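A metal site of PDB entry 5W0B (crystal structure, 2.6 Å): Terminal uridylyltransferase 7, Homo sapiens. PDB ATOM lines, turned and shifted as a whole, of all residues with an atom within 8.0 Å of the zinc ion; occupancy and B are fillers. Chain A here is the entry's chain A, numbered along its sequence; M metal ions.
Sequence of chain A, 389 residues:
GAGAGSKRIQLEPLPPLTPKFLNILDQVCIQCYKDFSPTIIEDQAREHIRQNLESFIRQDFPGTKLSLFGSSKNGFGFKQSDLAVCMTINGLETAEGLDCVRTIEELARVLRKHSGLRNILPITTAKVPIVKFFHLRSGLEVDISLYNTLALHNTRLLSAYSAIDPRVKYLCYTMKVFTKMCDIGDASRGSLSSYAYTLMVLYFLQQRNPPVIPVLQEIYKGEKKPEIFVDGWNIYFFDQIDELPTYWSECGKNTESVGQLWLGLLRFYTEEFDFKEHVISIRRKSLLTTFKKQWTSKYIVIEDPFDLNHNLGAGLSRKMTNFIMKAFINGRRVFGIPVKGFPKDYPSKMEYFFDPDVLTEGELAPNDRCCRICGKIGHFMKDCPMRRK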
ATOM      1  N   CYS A 370       4.178 -12.154   3.824  1.00  0.00           N
ATOM      2  CA  CYS A 370       4.883 -12.872   2.776  1.00  0.00           C
ATOM      3  C   CYS A 370       3.934 -13.624   1.850  1.00  0.00           C
ATOM      4  O   CYS A 370       2.894 -14.136   2.281  1.00  0.00           O
ATOM      5  CB  CYS A 370       5.880 -13.851   3.398  1.00  0.00           C
ATOM      6  SG  CYS A 370       7.015 -13.089   4.570  1.00  0.00           S
ATOM      7  N   CYS A 371       4.305 -13.673   0.586  1.00  0.00           N
ATOM      8  CA  CYS A 371       3.659 -14.545  -0.393  1.00  0.00           C
ATOM      9  C   CYS A 371       3.543 -15.955   0.163  1.00  0.00           C
ATOM     10  O   CYS A 371       4.549 -16.558   0.547  1.00  0.00           O
ATOM     11  CB  CYS A 371       4.497 -14.549  -1.675  1.00  0.00           C
ATOM     12  SG  CYS A 371       3.595 -14.734  -3.225  1.00  0.00           S
ATOM     13  N   ARG A 372       2.323 -16.476   0.209  1.00  0.00           N
ATOM     14  CA  ARG A 372       2.116 -17.823   0.750  1.00  0.00           C
ATOM     15  C   ARG A 372       2.684 -18.910  -0.153  1.00  0.00           C
ATOM     16  O   ARG A 372       2.592 -20.090   0.199  1.00  0.00           O
ATOM     17  CB  ARG A 372       0.628 -18.095   0.973  1.00  0.00           C
ATOM     18  CG  ARG A 372       0.031 -17.303   2.118  1.00  0.00           C
ATOM     19  CD  ARG A 372      -1.410 -17.722   2.338  1.00  0.00           C
ATOM     20  NE  ARG A 372      -2.058 -16.923   3.376  1.00  0.00           N
ATOM     21  CZ  ARG A 372      -3.336 -17.033   3.712  1.00  0.00           C
ATOM     22  NH1 ARG A 372      -4.119 -17.911   3.103  1.00  0.00           N
ATOM     23  NH2 ARG A 372      -3.829 -16.263   4.672  1.00  0.00           N
ATOM     24  N   ILE A 373       3.260 -18.548  -1.300  1.00  0.00           N
ATOM     25  CA  ILE A 373       3.880 -19.521  -2.206  1.00  0.00           C
ATOM     26  C   ILE A 373       5.397 -19.452  -2.105  1.00  0.00           C
ATOM     27  O   ILE A 373       6.056 -20.462  -1.881  1.00  0.00           O
ATOM     28  CB  ILE A 373       3.377 -19.304  -3.658  1.00  0.00           C
ATOM     29  CG1 ILE A 373       4.430 -19.652  -4.712  1.00  0.00           C
ATOM     30  CG2 ILE A 373       2.929 -17.891  -3.901  1.00  0.00           C
ATOM     31  CD1 ILE A 373       4.810 -21.065  -4.733  1.00  0.00           C
ATOM     32  N   CYS A 374       5.979 -18.253  -2.245  1.00  0.00           N
ATOM     33  CA  CYS A 374       7.425 -18.100  -2.130  1.00  0.00           C
ATOM     34  C   CYS A 374       7.875 -17.843  -0.702  1.00  0.00           C
ATOM     35  O   CYS A 374       8.968 -18.270  -0.310  1.00  0.00           O
ATOM     36  CB  CYS A 374       7.914 -16.955  -3.023  1.00  0.00           C
ATOM     37  SG  CYS A 374       7.632 -15.318  -2.334  1.00  0.00           S
ATOM     38  N   GLY A 375       7.070 -17.140   0.093  1.00  0.00           N
ATOM     39  CA  GLY A 375       7.456 -16.778   1.435  1.00  0.00           C
ATOM     40  C   GLY A 375       8.321 -15.541   1.542  1.00  0.00           C
ATOM     41  O   GLY A 375       8.889 -15.290   2.612  1.00  0.00           O
ATOM     42  N   LYS A 376       8.438 -14.761   0.467  1.00  0.00           N
ATOM     43  CA  LYS A 376       9.226 -13.533   0.458  1.00  0.00           C
ATOM     44  C   LYS A 376       8.301 -12.330   0.390  1.00  0.00           C
ATOM     45  O   LYS A 376       7.198 -12.393  -0.174  1.00  0.00           O
ATOM     46  CB  LYS A 376      10.186 -13.501  -0.725  1.00  0.00           C
ATOM     47  CG  LYS A 376      11.332 -14.500  -0.643  1.00  0.00           C
ATOM     48  CD  LYS A 376      12.305 -14.313  -1.799  1.00  0.00           C
ATOM     49  CE  LYS A 376      13.512 -15.217  -1.672  1.00  0.00           C
ATOM     50  NZ  LYS A 376      14.477 -15.000  -2.784  1.00  0.00           N
ATOM     51  N   ILE A 377       8.752 -11.222   0.969  1.00  0.00           N
ATOM     52  CA  ILE A 377       7.999  -9.976   0.898  1.00  0.00           C
ATOM     53  C   ILE A 377       8.338  -9.257  -0.405  1.00  0.00           C
ATOM     54  O   ILE A 377       9.345  -9.523  -1.060  1.00  0.00           O
ATOM     55  CB  ILE A 377       8.274  -9.078   2.125  1.00  0.00           C
ATOM     56  CG1 ILE A 377       9.701  -8.496   2.079  1.00  0.00           C
ATOM     57  CG2 ILE A 377       8.076  -9.865   3.420  1.00  0.00           C
ATOM     58  CD1 ILE A 377       9.934  -7.388   3.075  1.00  0.00           C
ATOM     59  N   GLY A 378       7.471  -8.310  -0.773  1.00  0.00           N
ATOM     60  CA  GLY A 378       7.704  -7.462  -1.924  1.00  0.00           C
ATOM     61  C   GLY A 378       6.700  -7.603  -3.053  1.00  0.00           C
ATOM     62  O   GLY A 378       6.697  -6.769  -3.971  1.00  0.00           O
ATOM     63  N   HIS A 379       5.835  -8.623  -3.031  1.00  0.00           N
ATOM     64  CA  HIS A 379       4.858  -8.797  -4.096  1.00  0.00           C
ATOM     65  C   HIS A 379       3.667  -9.574  -3.552  1.00  0.00           C
ATOM     66  O   HIS A 379       3.789 -10.357  -2.605  1.00  0.00           O
ATOM     67  CB  HIS A 379       5.452  -9.520  -5.301  1.00  0.00           C
ATOM     68  CG  HIS A 379       6.049 -10.864  -4.976  1.00  0.00           C
ATOM     69  ND1 HIS A 379       7.310 -11.001  -4.462  1.00  0.00           N
ATOM     70  CD2 HIS A 379       5.538 -12.106  -5.086  1.00  0.00           C
ATOM     71  CE1 HIS A 379       7.563 -12.286  -4.271  1.00  0.00           C
ATOM     72  NE2 HIS A 379       6.504 -12.985  -4.640  1.00  0.00           N
ATOM     73  N   PHE A 380       2.517  -9.359  -4.188  1.00  0.00           N
ATOM     74  CA  PHE A 380       1.321 -10.121  -3.845  1.00  0.00           C
ATOM     75  C   PHE A 380       1.435 -11.534  -4.414  1.00  0.00           C
ATOM     76  O   PHE A 380       2.438 -11.916  -5.026  1.00  0.00           O
ATOM     77  CB  PHE A 380       0.071  -9.424  -4.386  1.00  0.00           C
ATOM     78  CG  PHE A 380       0.109  -7.922  -4.243  1.00  0.00           C
ATOM     79  CD1 PHE A 380      -0.153  -7.319  -3.027  1.00  0.00           C
ATOM     80  CD2 PHE A 380       0.401  -7.124  -5.343  1.00  0.00           C
ATOM     81  CE1 PHE A 380      -0.119  -5.938  -2.906  1.00  0.00           C
ATOM     82  CE2 PHE A 380       0.434  -5.742  -5.222  1.00  0.00           C
ATOM     83  CZ  PHE A 380       0.177  -5.159  -4.001  1.00  0.00           C
ATOM     84  N   MET A 381       0.388 -12.328  -4.206  1.00  0.00           N
ATOM     85  CA  MET A 381       0.398 -13.720  -4.642  1.00  0.00           C
ATOM     86  C   MET A 381       0.191 -13.886  -6.147  1.00  0.00           C
ATOM     87  O   MET A 381       0.301 -15.009  -6.634  1.00  0.00           O
ATOM     88  CB  MET A 381      -0.673 -14.511  -3.893  1.00  0.00           C
ATOM     89  CG  MET A 381      -0.636 -14.358  -2.386  1.00  0.00           C
ATOM     90  SD  MET A 381      -1.868 -15.382  -1.560  1.00  0.00           S
ATOM     91  CE  MET A 381      -1.331 -17.014  -2.036  1.00  0.00           C
ATOM     92  N   LYS A 382      -0.099 -12.804  -6.877  1.00  0.00           N
ATOM     93  CA  LYS A 382      -0.409 -12.936  -8.288  1.00  0.00           C
ATOM     94  C   LYS A 382       0.824 -12.785  -9.186  1.00  0.00           C
ATOM     95  O   LYS A 382       0.879 -13.424 -10.246  1.00  0.00           O
ATOM     96  CB  LYS A 382      -1.477 -11.902  -8.699  1.00  0.00           C
ATOM     97  CG  LYS A 382      -0.982 -10.696  -9.512  1.00  0.00           C
ATOM     98  CD  LYS A 382      -2.157  -9.922 -10.099  1.00  0.00           C
ATOM     99  CE  LYS A 382      -1.710  -9.084 -11.294  1.00  0.00           C
ATOM    100  NZ  LYS A 382      -2.864  -8.571 -12.081  1.00  0.00           N
ATOM    101  N   ASP A 383       1.813 -11.986  -8.778  1.00  0.00           N
ATOM    102  CA  ASP A 383       2.972 -11.700  -9.615  1.00  0.00           C
ATOM    103  C   ASP A 383       4.221 -12.462  -9.175  1.00  0.00           C
ATOM    104  O   ASP A 383       5.335 -11.963  -9.360  1.00  0.00           O
ATOM    105  CB  ASP A 383       3.261 -10.203  -9.615  1.00  0.00           C
ATOM    106  CG  ASP A 383       2.096  -9.373 -10.107  1.00  0.00           C
ATOM    107  OD1 ASP A 383       1.872  -9.333 -11.340  1.00  0.00           O
ATOM    108  OD2 ASP A 383       1.411  -8.753  -9.271  1.00  0.00           O
ATOM    109  N   CYS A 384       4.059 -13.669  -8.606  1.00  0.00           N
ATOM    110  CA  CYS A 384       5.254 -14.352  -8.138  1.00  0.00           C
ATOM    111  C   CYS A 384       5.817 -15.270  -9.213  1.00  0.00           C
ATOM    112  O   CYS A 384       5.061 -15.867  -9.987  1.00  0.00           O
ATOM    113  CB  CYS A 384       4.941 -15.171  -6.885  1.00  0.00           C
ATOM    114  SG  CYS A 384       6.416 -15.813  -6.069  1.00  0.00           S
ATOM    115  N   PRO A 385       7.158 -15.403  -9.298  1.00  0.00           N
ATOM    116  CA  PRO A 385       7.774 -16.410 -10.165  1.00  0.00           C
ATOM    117  C   PRO A 385       7.232 -17.819  -9.927  1.00  0.00           C
ATOM    118  O   PRO A 385       6.096 -18.118 -10.307  1.00  0.00           O
ATOM    119  CB  PRO A 385       9.252 -16.347  -9.783  1.00  0.00           C
ATOM    120  CG  PRO A 385       9.462 -15.024  -9.107  1.00  0.00           C
ATOM    121  CD  PRO A 385       8.127 -14.385  -8.868  1.00  0.00           C
HETATM  122 ZN    ZN M   1       5.975 -14.827  -3.932  1.00  0.00          ZN
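NE2 of His 379 binds the zinc ion (2.0 Å).
The side-chain sulfur (SG) of Cys 374 is bound to the zinc ion.
The zinc ion is bound by SG of Cys 384.
The side-chain sulfur (SG) of Cys 371 is bound to the zinc ion (2.5 Å).
The zinc ion has four donor atoms within binding distance.
The side-chain sulfur of Cys 374 lies close to the backbone NH of Lys 376 (3.0 Å).
The backbone NH (N) of Cys 371 sits at hydrogen-bond distance from the backbone carbonyl oxygen (O) of Lys 376 (3.3 Å).
The backbone carbonyl oxygen (O) of Phe 380 lies close to the side-chain sulfur (SG) of Cys 371 (3.5 Å).
Four residues have an atom within 4 Å of the zinc ion: Cys 371, Cys 374, His 379 and Cys 384.
The nearest printed residue that does not touch the zinc ion is Ile 373 (4.3 Å).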
